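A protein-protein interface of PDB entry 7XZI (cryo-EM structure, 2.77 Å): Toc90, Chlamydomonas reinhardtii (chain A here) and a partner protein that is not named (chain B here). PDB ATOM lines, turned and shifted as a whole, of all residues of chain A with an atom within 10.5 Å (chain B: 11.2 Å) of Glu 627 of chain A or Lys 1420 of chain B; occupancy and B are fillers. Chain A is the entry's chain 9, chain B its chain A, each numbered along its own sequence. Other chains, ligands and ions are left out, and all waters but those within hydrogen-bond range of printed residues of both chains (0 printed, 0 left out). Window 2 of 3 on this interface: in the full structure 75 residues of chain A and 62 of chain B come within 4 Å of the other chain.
NZ of Lys 1421 of chain B lies within salt-bridge range of OE2 of Glu 627 of chain A (3.9 Å). The backbone NH of Gly 1378 of chain B lies within hydrogen-bond range of the backbone carbonyl oxygen of Glu 623 of chain A (3.1 Å).
The side-chain hydroxyl (OH) of Tyr 624 of chain A lies within hydrogen-bond range of the side-chain carboxylate (OE2) of Glu 623 of chain A. O of Gly 625 of chain A lies within hydrogen-bond range of ND2 of Asn 621 of chain A.
Among the printed residues, merely in contact across the chains: Asn 621 of chain A with Leu 1405 of chain B, Tyr 624 of chain A with Ser 1422 of chain B, Gly 625 of chain A with Lys 1421 of chain B, Glu 627 of chain A with Lys 1420 of chain B, Val 630 of chain A with Ser 1422 of chain B and Val 630 of chain A with Gln 1423 of chain B.
Printed residues of chain B within 4 Å of Asn 621 of chain A: Leu 1405 (3.3 Å). Of chain B, only Lys 1421 comes within 4 Å of Gly 625 of chain A. No residue of chain B comes within 4 Å of Val 626 of chain A. Glu 627 of chain A touches just these residues of chain B: Lys 1420 (3.9 Å) and Lys 1421 (2.8 Å). No residue of chain B comes within 4 Å of Ser 628 of chain A. Printed residues of chain A within 4 Å of Gly 1378 of chain B: Glu 623 (3.1 Å). Of the printed residues of chain A, Leu 1405 of chain B touches Asn 621. Ser 1418 of chain B touches none of the printed residues of chain A. Leu 1419 of chain B touches none of the printed residues of chain A. The nearest residue of chain B that does not touch Glu 627 of chain A is Leu 1419 of chain B (4.4 Å).
Of the 19 printed residues of chain B, 6 touch a printed residue of chain A. Hydrophobic or aromatic side chains of chain B within 4 Å of the printed part of chain A: Leu 1405. Printed residues of chain A that touch a printed residue of chain B: Asn 621, Glu 623, Tyr 624, Gly 625, Glu 627 and Val 630. Hydrophobic or aromatic side chains of chain A within 4 Å of the printed part of chain B: Tyr 624 and Val 630. Among the printed residues, 8 pairs touch across the chains. Among the printed residues, Asp or Glu carboxylates within 4 Å of a Lys or Arg side-chain nitrogen of the other chain: Glu 627 of chain A with Lys 1421 of chain B.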
ATOM      1  N   ASP A 617     -13.733 -18.296   9.633  1.00  0.00           N
ATOM      2  CA  ASP A 617     -13.552 -16.988  10.256  1.00  0.00           C
ATOM      3  C   ASP A 617     -13.400 -17.115  11.767  1.00  0.00           C
ATOM      4  O   ASP A 617     -12.555 -16.443  12.375  1.00  0.00           O
ATOM      5  CB  ASP A 617     -14.723 -16.069   9.909  1.00  0.00           C
ATOM      6  CG  ASP A 617     -14.535 -14.661  10.440  1.00  0.00           C
ATOM      7  OD1 ASP A 617     -13.633 -13.954   9.942  1.00  0.00           O
ATOM      8  OD2 ASP A 617     -15.286 -14.262  11.354  1.00  0.00           O
ATOM      9  N   ASP A 619     -12.246 -19.720  13.416  1.00  0.00           N
ATOM     10  CA  ASP A 619     -10.931 -20.298  13.681  1.00  0.00           C
ATOM     11  C   ASP A 619      -9.824 -19.265  13.509  1.00  0.00           C
ATOM     12  O   ASP A 619      -8.869 -19.229  14.296  1.00  0.00           O
ATOM     13  CB  ASP A 619     -10.688 -21.498  12.766  1.00  0.00           C
ATOM     14  CG  ASP A 619      -9.284 -22.054  12.899  1.00  0.00           C
ATOM     15  OD1 ASP A 619      -8.977 -22.654  13.950  1.00  0.00           O
ATOM     16  OD2 ASP A 619      -8.486 -21.889  11.952  1.00  0.00           O
ATOM     17  N   ALA A 620      -9.926 -18.424  12.476  1.00  0.00           N
ATOM     18  CA  ALA A 620      -8.929 -17.380  12.270  1.00  0.00           C
ATOM     19  C   ALA A 620      -8.920 -16.395  13.431  1.00  0.00           C
ATOM     20  O   ALA A 620      -7.855 -15.945  13.866  1.00  0.00           O
ATOM     21  CB  ALA A 620      -9.188 -16.658  10.948  1.00  0.00           C
ATOM     22  N   ASN A 621     -10.103 -16.041  13.940  1.00  0.00           N
ATOM     23  CA  ASN A 621     -10.171 -15.197  15.129  1.00  0.00           C
ATOM     24  C   ASN A 621      -9.559 -15.887  16.343  1.00  0.00           C
ATOM     25  O   ASN A 621      -8.904 -15.234  17.164  1.00  0.00           O
ATOM     26  CB  ASN A 621     -11.620 -14.806  15.416  1.00  0.00           C
ATOM     27  CG  ASN A 621     -11.785 -14.121  16.759  1.00  0.00           C
ATOM     28  OD1 ASN A 621     -12.089 -14.764  17.764  1.00  0.00           O
ATOM     29  ND2 ASN A 621     -11.582 -12.809  16.784  1.00  0.00           N
ATOM     30  N   VAL A 622      -9.770 -17.196  16.479  1.00  0.00           N
ATOM     31  CA  VAL A 622      -9.244 -17.927  17.631  1.00  0.00           C
ATOM     32  C   VAL A 622      -7.720 -17.952  17.600  1.00  0.00           C
ATOM     33  O   VAL A 622      -7.059 -17.715  18.618  1.00  0.00           O
ATOM     34  CB  VAL A 622      -9.829 -19.350  17.683  1.00  0.00           C
ATOM     35  CG1 VAL A 622      -9.056 -20.208  18.673  1.00  0.00           C
ATOM     36  CG2 VAL A 622     -11.301 -19.305  18.062  1.00  0.00           C
ATOM     37  N   GLU A 623      -7.141 -18.249  16.433  1.00  0.00           N
ATOM     38  CA  GLU A 623      -5.686 -18.332  16.325  1.00  0.00           C
ATOM     39  C   GLU A 623      -5.033 -16.993  16.654  1.00  0.00           C
ATOM     40  O   GLU A 623      -4.263 -16.879  17.614  1.00  0.00           O
ATOM     41  CB  GLU A 623      -5.282 -18.798  14.924  1.00  0.00           C
ATOM     42  CG  GLU A 623      -3.784 -19.030  14.770  1.00  0.00           C
ATOM     43  CD  GLU A 623      -3.402 -19.508  13.383  1.00  0.00           C
ATOM     44  OE1 GLU A 623      -4.289 -19.560  12.505  1.00  0.00           O
ATOM     45  OE2 GLU A 623      -2.215 -19.832  13.170  1.00  0.00           O
ATOM     46  N   TYR A 624      -5.332 -15.967  15.864  1.00  0.00           N
ATOM     47  CA  TYR A 624      -4.864 -14.612  16.119  1.00  0.00           C
ATOM     48  C   TYR A 624      -6.053 -13.788  16.592  1.00  0.00           C
ATOM     49  O   TYR A 624      -7.005 -13.578  15.833  1.00  0.00           O
ATOM     50  CB  TYR A 624      -4.239 -13.995  14.868  1.00  0.00           C
ATOM     51  CG  TYR A 624      -3.312 -14.924  14.117  1.00  0.00           C
ATOM     52  CD1 TYR A 624      -2.036 -15.196  14.589  1.00  0.00           C
ATOM     53  CD2 TYR A 624      -3.712 -15.521  12.929  1.00  0.00           C
ATOM     54  CE1 TYR A 624      -1.185 -16.043  13.903  1.00  0.00           C
ATOM     55  CE2 TYR A 624      -2.868 -16.368  12.235  1.00  0.00           C
ATOM     56  CZ  TYR A 624      -1.606 -16.625  12.726  1.00  0.00           C
ATOM     57  OH  TYR A 624      -0.760 -17.467  12.041  1.00  0.00           O
ATOM     58  N   GLY A 625      -5.992 -13.322  17.841  1.00  0.00           N
ATOM     59  CA  GLY A 625      -7.157 -12.692  18.442  1.00  0.00           C
ATOM     60  C   GLY A 625      -7.609 -11.451  17.697  1.00  0.00           C
ATOM     61  O   GLY A 625      -8.794 -11.291  17.394  1.00  0.00           O
ATOM     62  N   VAL A 626      -6.673 -10.555  17.393  1.00  0.00           N
ATOM     63  CA  VAL A 626      -7.004  -9.317  16.696  1.00  0.00           C
ATOM     64  C   VAL A 626      -6.029  -9.081  15.551  1.00  0.00           C
ATOM     65  O   VAL A 626      -6.285  -8.258  14.666  1.00  0.00           O
ATOM     66  CB  VAL A 626      -7.009  -8.122  17.666  1.00  0.00           C
ATOM     67  CG1 VAL A 626      -8.245  -8.161  18.552  1.00  0.00           C
ATOM     68  CG2 VAL A 626      -5.747  -8.127  18.512  1.00  0.00           C
ATOM     69  N   GLU A 627      -4.915  -9.809  15.553  1.00  0.00           N
ATOM     70  CA  GLU A 627      -3.836  -9.567  14.600  1.00  0.00           C
ATOM     71  C   GLU A 627      -4.215 -10.136  13.237  1.00  0.00           C
ATOM     72  O   GLU A 627      -4.398 -11.348  13.089  1.00  0.00           O
ATOM     73  CB  GLU A 627      -2.532 -10.178  15.102  1.00  0.00           C
ATOM     74  CG  GLU A 627      -2.018  -9.567  16.393  1.00  0.00           C
ATOM     75  CD  GLU A 627      -0.553  -9.194  16.313  1.00  0.00           C
ATOM     76  OE1 GLU A 627      -0.065  -8.934  15.193  1.00  0.00           O
ATOM     77  OE2 GLU A 627       0.113  -9.162  17.370  1.00  0.00           O
ATOM     78  N   SER A 628      -4.334  -9.261  12.242  1.00  0.00           N
ATOM     79  CA  SER A 628      -4.575  -9.706  10.878  1.00  0.00           C
ATOM     80  C   SER A 628      -3.318 -10.348  10.297  1.00  0.00           C
ATOM     81  O   SER A 628      -2.191  -9.969  10.625  1.00  0.00           O
ATOM     82  CB  SER A 628      -5.021  -8.536  10.002  1.00  0.00           C
ATOM     83  OG  SER A 628      -4.040  -7.515   9.973  1.00  0.00           O
ATOM     84  N   TYR A 629      -3.527 -11.335   9.428  1.00  0.00           N
ATOM     85  CA  TYR A 629      -2.409 -12.050   8.827  1.00  0.00           C
ATOM     86  C   TYR A 629      -1.607 -11.128   7.915  1.00  0.00           C
ATOM     87  O   TYR A 629      -2.167 -10.318   7.173  1.00  0.00           O
ATOM     88  CB  TYR A 629      -2.922 -13.259   8.045  1.00  0.00           C
ATOM     89  CG  TYR A 629      -1.833 -14.153   7.500  1.00  0.00           C
ATOM     90  CD1 TYR A 629      -1.063 -14.937   8.349  1.00  0.00           C
ATOM     91  CD2 TYR A 629      -1.582 -14.223   6.136  1.00  0.00           C
ATOM     92  CE1 TYR A 629      -0.069 -15.758   7.856  1.00  0.00           C
ATOM     93  CE2 TYR A 629      -0.592 -15.044   5.634  1.00  0.00           C
ATOM     94  CZ  TYR A 629       0.163 -15.809   6.498  1.00  0.00           C
ATOM     95  OH  TYR A 629       1.152 -16.626   6.003  1.00  0.00           O
ATOM     96  N   VAL A 630      -0.285 -11.260   7.974  1.00  0.00           N
ATOM     97  CA  VAL A 630       0.620 -10.440   7.181  1.00  0.00           C
ATOM     98  C   VAL A 630       1.156 -11.275   6.025  1.00  0.00           C
ATOM     99  O   VAL A 630       1.135 -12.510   6.048  1.00  0.00           O
ATOM    100  CB  VAL A 630       1.775  -9.869   8.028  1.00  0.00           C
ATOM    101  CG1 VAL A 630       1.231  -8.960   9.119  1.00  0.00           C
ATOM    102  CG2 VAL A 630       2.601 -10.995   8.628  1.00  0.00           C
ATOM    103  N   VAL A 631       1.646 -10.584   4.999  1.00  0.00           N
ATOM    104  CA  VAL A 631       2.098 -11.231   3.775  1.00  0.00           C
ATOM    105  C   VAL A 631       3.613 -11.102   3.663  1.00  0.00           C
ATOM    106  O   VAL A 631       4.230 -10.161   4.172  1.00  0.00           O
ATOM    107  CB  VAL A 631       1.397 -10.648   2.528  1.00  0.00           C
ATOM    108  CG1 VAL A 631       1.966  -9.281   2.176  1.00  0.00           C
ATOM    109  CG2 VAL A 631       1.502 -11.607   1.350  1.00  0.00           C
ATOM    110  N   TYR A 652       2.240  -6.155   4.025  1.00  0.00           N
ATOM    111  CA  TYR A 652       0.912  -5.623   4.281  1.00  0.00           C
ATOM    112  C   TYR A 652      -0.007  -6.725   4.794  1.00  0.00           C
ATOM    113  O   TYR A 652       0.261  -7.919   4.634  1.00  0.00           O
ATOM    114  CB  TYR A 652       0.321  -4.978   3.019  1.00  0.00           C
ATOM    115  CG  TYR A 652       0.325  -5.873   1.798  1.00  0.00           C
ATOM    116  CD1 TYR A 652      -0.734  -6.734   1.539  1.00  0.00           C
ATOM    117  CD2 TYR A 652       1.384  -5.851   0.899  1.00  0.00           C
ATOM    118  CE1 TYR A 652      -0.734  -7.551   0.423  1.00  0.00           C
ATOM    119  CE2 TYR A 652       1.392  -6.664  -0.219  1.00  0.00           C
ATOM    120  CZ  TYR A 652       0.330  -7.512  -0.451  1.00  0.00           C
ATOM    121  OH  TYR A 652       0.331  -8.323  -1.563  1.00  0.00           O
ATOM    122  N   ALA A 653      -1.100  -6.305   5.424  1.00  0.00           N
ATOM    123  CA  ALA A 653      -2.098  -7.249   5.906  1.00  0.00           C
ATOM    124  C   ALA A 653      -2.786  -7.935   4.733  1.00  0.00           C
ATOM    125  O   ALA A 653      -3.018  -7.325   3.685  1.00  0.00           O
ATOM    126  CB  ALA A 653      -3.129  -6.535   6.779  1.00  0.00           C
ATOM    127  N   GLU A 654      -3.103  -9.216   4.912  1.00  0.00           N
ATOM    128  CA  GLU A 654      -3.755  -9.981   3.857  1.00  0.00           C
ATOM    129  C   GLU A 654      -5.112  -9.376   3.519  1.00  0.00           C
ATOM    130  O   GLU A 654      -5.909  -9.068   4.410  1.00  0.00           O
ATOM    131  CB  GLU A 654      -3.916 -11.440   4.287  1.00  0.00           C
ATOM    132  N   LYS B1373       6.382 -26.147  14.913  1.00  0.00           N
ATOM    133  CA  LYS B1373       6.786 -25.708  16.238  1.00  0.00           C
ATOM    134  C   LYS B1373       5.562 -25.423  17.094  1.00  0.00           C
ATOM    135  O   LYS B1373       4.620 -24.771  16.623  1.00  0.00           O
ATOM    136  CB  LYS B1373       7.667 -24.454  16.152  1.00  0.00           C
ATOM    137  CG  LYS B1373       7.058 -23.305  15.362  1.00  0.00           C
ATOM    138  CD  LYS B1373       7.952 -22.077  15.393  1.00  0.00           C
ATOM    139  CE  LYS B1373       8.170 -21.587  16.815  1.00  0.00           C
ATOM    140  NZ  LYS B1373       6.891 -21.205  17.475  1.00  0.00           N
ATOM    141  N   ARG B1375       3.124 -23.602  19.730  1.00  0.00           N
ATOM    142  CA  ARG B1375       2.911 -22.185  19.979  1.00  0.00           C
ATOM    143  C   ARG B1375       1.644 -22.013  20.803  1.00  0.00           C
ATOM    144  O   ARG B1375       0.823 -22.926  20.922  1.00  0.00           O
ATOM    145  CB  ARG B1375       2.817 -21.396  18.669  1.00  0.00           C
ATOM    146  CG  ARG B1375       1.478 -21.541  17.965  1.00  0.00           C
ATOM    147  CD  ARG B1375       1.643 -21.582  16.456  1.00  0.00           C
ATOM    148  NE  ARG B1375       2.354 -22.778  16.026  1.00  0.00           N
ATOM    149  CZ  ARG B1375       2.540 -23.126  14.757  1.00  0.00           C
ATOM    150  NH1 ARG B1375       2.078 -22.387  13.762  1.00  0.00           N
ATOM    151  NH2 ARG B1375       3.204 -24.245  14.482  1.00  0.00           N
ATOM    152  N   LEU B1376       1.494 -20.823  21.377  1.00  0.00           N
ATOM    153  CA  LEU B1376       0.323 -20.474  22.168  1.00  0.00           C
ATOM    154  C   LEU B1376      -0.631 -19.623  21.341  1.00  0.00           C
ATOM    155  O   LEU B1376      -0.205 -18.708  20.630  1.00  0.00           O
ATOM    156  CB  LEU B1376       0.723 -19.720  23.438  1.00  0.00           C
ATOM    157  CG  LEU B1376       1.640 -20.460  24.414  1.00  0.00           C
ATOM    158  CD1 LEU B1376       1.848 -19.645  25.683  1.00  0.00           C
ATOM    159  CD2 LEU B1376       1.073 -21.831  24.738  1.00  0.00           C
ATOM    160  N   VAL B1377      -1.925 -19.934  21.435  1.00  0.00           N
ATOM    161  CA  VAL B1377      -2.922 -19.123  20.748  1.00  0.00           C
ATOM    162  C   VAL B1377      -3.012 -17.750  21.407  1.00  0.00           C
ATOM    163  O   VAL B1377      -2.686 -17.565  22.586  1.00  0.00           O
ATOM    164  CB  VAL B1377      -4.293 -19.819  20.729  1.00  0.00           C
ATOM    165  CG1 VAL B1377      -4.179 -21.205  20.116  1.00  0.00           C
ATOM    166  CG2 VAL B1377      -4.876 -19.893  22.132  1.00  0.00           C
ATOM    167  N   GLY B1378      -3.457 -16.768  20.623  1.00  0.00           N
ATOM    168  CA  GLY B1378      -3.619 -15.429  21.164  1.00  0.00           C
ATOM    169  C   GLY B1378      -4.742 -15.335  22.176  1.00  0.00           C
ATOM    170  O   GLY B1378      -4.747 -14.440  23.025  1.00  0.00           O
ATOM    171  N   LEU B1379      -5.710 -16.250  22.095  1.00  0.00           N
ATOM    172  CA  LEU B1379      -6.847 -16.217  23.010  1.00  0.00           C
ATOM    173  C   LEU B1379      -6.426 -16.537  24.440  1.00  0.00           C
ATOM    174  O   LEU B1379      -6.743 -15.791  25.373  1.00  0.00           O
ATOM    175  CB  LEU B1379      -7.923 -17.191  22.529  1.00  0.00           C
ATOM    176  CG  LEU B1379      -9.107 -17.425  23.466  1.00  0.00           C
ATOM    177  N   LEU B1405     -13.421 -17.702  23.638  1.00  0.00           N
ATOM    178  CA  LEU B1405     -13.549 -16.369  23.060  1.00  0.00           C
ATOM    179  C   LEU B1405     -14.402 -15.470  23.947  1.00  0.00           C
ATOM    180  O   LEU B1405     -14.053 -14.311  24.196  1.00  0.00           O
ATOM    181  CB  LEU B1405     -14.143 -16.464  21.654  1.00  0.00           C
ATOM    182  CG  LEU B1405     -14.446 -15.139  20.953  1.00  0.00           C
ATOM    183  CD1 LEU B1405     -13.189 -14.289  20.843  1.00  0.00           C
ATOM    184  CD2 LEU B1405     -15.056 -15.380  19.579  1.00  0.00           C
ATOM    185  N   GLU B1414      -4.263  -6.596  28.589  1.00  0.00           N
ATOM    186  CA  GLU B1414      -3.033  -6.543  27.791  1.00  0.00           C
ATOM    187  C   GLU B1414      -3.313  -6.029  26.376  1.00  0.00           C
ATOM    188  O   GLU B1414      -3.146  -6.747  25.390  1.00  0.00           O
ATOM    189  CB  GLU B1414      -2.340  -7.909  27.754  1.00  0.00           C
ATOM    190  N   LEU B1415      -3.743  -4.768  26.289  1.00  0.00           N
ATOM    191  CA  LEU B1415      -4.117  -4.185  25.004  1.00  0.00           C
ATOM    192  C   LEU B1415      -2.941  -4.167  24.032  1.00  0.00           C
ATOM    193  O   LEU B1415      -3.063  -4.591  22.877  1.00  0.00           O
ATOM    194  CB  LEU B1415      -4.666  -2.772  25.215  1.00  0.00           C
ATOM    195  N   THR B1416      -1.786  -3.679  24.484  1.00  0.00           N
ATOM    196  CA  THR B1416      -0.625  -3.536  23.615  1.00  0.00           C
ATOM    197  C   THR B1416       0.626  -4.238  24.127  1.00  0.00           C
ATOM    198  O   THR B1416       1.359  -4.817  23.320  1.00  0.00           O
ATOM    199  CB  THR B1416      -0.305  -2.048  23.394  1.00  0.00           C
ATOM    200  OG1 THR B1416      -1.489  -1.363  22.968  1.00  0.00           O
ATOM    201  CG2 THR B1416       0.772  -1.876  22.330  1.00  0.00           C
ATOM    202  N   ASN B1417       0.881  -4.223  25.433  1.00  0.00           N
ATOM    203  CA  ASN B1417       2.101  -4.805  25.996  1.00  0.00           C
ATOM    204  C   ASN B1417       1.967  -6.322  25.982  1.00  0.00           C
ATOM    205  O   ASN B1417       1.549  -6.944  26.960  1.00  0.00           O
ATOM    206  N   SER B1418       2.330  -6.926  24.854  1.00  0.00           N
ATOM    207  CA  SER B1418       2.278  -8.373  24.702  1.00  0.00           C
ATOM    208  C   SER B1418       3.177  -8.770  23.541  1.00  0.00           C
ATOM    209  O   SER B1418       3.612  -7.931  22.751  1.00  0.00           O
ATOM    210  CB  SER B1418       0.843  -8.861  24.480  1.00  0.00           C
ATOM    211  OG  SER B1418       0.290  -8.288  23.308  1.00  0.00           O
ATOM    212  N   LEU B1419       3.453 -10.070  23.453  1.00  0.00           N
ATOM    213  CA  LEU B1419       4.243 -10.586  22.347  1.00  0.00           C
ATOM    214  C   LEU B1419       3.493 -10.401  21.030  1.00  0.00           C
ATOM    215  O   LEU B1419       2.260 -10.421  20.975  1.00  0.00           O
ATOM    216  CB  LEU B1419       4.577 -12.063  22.560  1.00  0.00           C
ATOM    217  CG  LEU B1419       5.729 -12.408  23.510  1.00  0.00           C
ATOM    218  CD1 LEU B1419       6.983 -11.624  23.143  1.00  0.00           C
ATOM    219  CD2 LEU B1419       5.351 -12.180  24.969  1.00  0.00           C
ATOM    220  N   LYS B1420       4.256 -10.215  19.958  1.00  0.00           N
ATOM    221  CA  LYS B1420       3.701  -9.908  18.647  1.00  0.00           C
ATOM    222  C   LYS B1420       3.400 -11.202  17.903  1.00  0.00           C
ATOM    223  O   LYS B1420       4.318 -11.946  17.542  1.00  0.00           O
ATOM    224  CB  LYS B1420       4.665  -9.038  17.840  1.00  0.00           C
ATOM    225  N   LYS B1421       2.116 -11.467  17.677  1.00  0.00           N
ATOM    226  CA  LYS B1421       1.702 -12.583  16.846  1.00  0.00           C
ATOM    227  C   LYS B1421       1.798 -12.201  15.372  1.00  0.00           C
ATOM    228  O   LYS B1421       1.843 -11.022  15.010  1.00  0.00           O
ATOM    229  CB  LYS B1421       0.278 -13.012  17.191  1.00  0.00           C
ATOM    230  CG  LYS B1421       0.099 -13.487  18.619  1.00  0.00           C
ATOM    231  CD  LYS B1421      -1.343 -13.877  18.880  1.00  0.00           C
ATOM    232  CE  LYS B1421      -2.281 -12.704  18.647  1.00  0.00           C
ATOM    233  NZ  LYS B1421      -1.976 -11.568  19.556  1.00  0.00           N
ATOM    234  N   SER B1422       1.817 -13.222  14.516  1.00  0.00           N
ATOM    235  CA  SER B1422       1.967 -13.038  13.073  1.00  0.00           C
ATOM    236  C   SER B1422       3.206 -12.199  12.767  1.00  0.00           C
ATOM    237  O   SER B1422       3.122 -11.081  12.254  1.00  0.00           O
ATOM    238  CB  SER B1422       0.711 -12.415  12.460  1.00  0.00           C
ATOM    239  OG  SER B1422      -0.416 -13.255  12.638  1.00  0.00           O
ATOM    240  N   GLN B1423       4.367 -12.751  13.113  1.00  0.00           N
ATOM    241  CA  GLN B1423       5.638 -12.056  12.951  1.00  0.00           C
ATOM    242  C   GLN B1423       5.838 -11.610  11.510  1.00  0.00           C
ATOM    243  O   GLN B1423       5.528 -12.342  10.568  1.00  0.00           O
ATOM    244  CB  GLN B1423       6.788 -12.970  13.387  1.00  0.00           C
ATOM    245  CG  GLN B1423       6.811 -14.309  12.675  1.00  0.00           C
ATOM    246  CD  GLN B1423       7.914 -15.219  13.170  1.00  0.00           C
ATOM    247  OE1 GLN B1423       8.753 -14.817  13.975  1.00  0.00           O
ATOM    248  NE2 GLN B1423       7.916 -16.457  12.691  1.00  0.00           N
ATOM    249  N   ILE B1424       6.345 -10.390  11.346  1.00  0.00           N
ATOM    250  CA  ILE B1424       6.539  -9.810  10.023  1.00  0.00           C
ATOM    251  C   ILE B1424       7.687 -10.533   9.339  1.00  0.00           C
ATOM    252  O   ILE B1424       8.855 -10.342   9.694  1.00  0.00           O
ATOM    253  CB  ILE B1424       6.807  -8.296  10.109  1.00  0.00           C
ATOM    254  CG1 ILE B1424       5.646  -7.587  10.812  1.00  0.00           C
ATOM    255  CG2 ILE B1424       7.033  -7.716   8.724  1.00  0.00           C
ATOM    256  CD1 ILE B1424       5.818  -6.087  10.906  1.00  0.00           C
ATOM    257  N   LYS B1425       7.363 -11.373   8.357  1.00  0.00           N
ATOM    258  CA  LYS B1425       8.387 -12.148   7.675  1.00  0.00           C
ATOM    259  C   LYS B1425       9.336 -11.228   6.920  1.00  0.00           C
ATOM    260  O   LYS B1425       8.910 -10.279   6.257  1.00  0.00           O
ATOM    261  CB  LYS B1425       7.744 -13.152   6.718  1.00  0.00           C
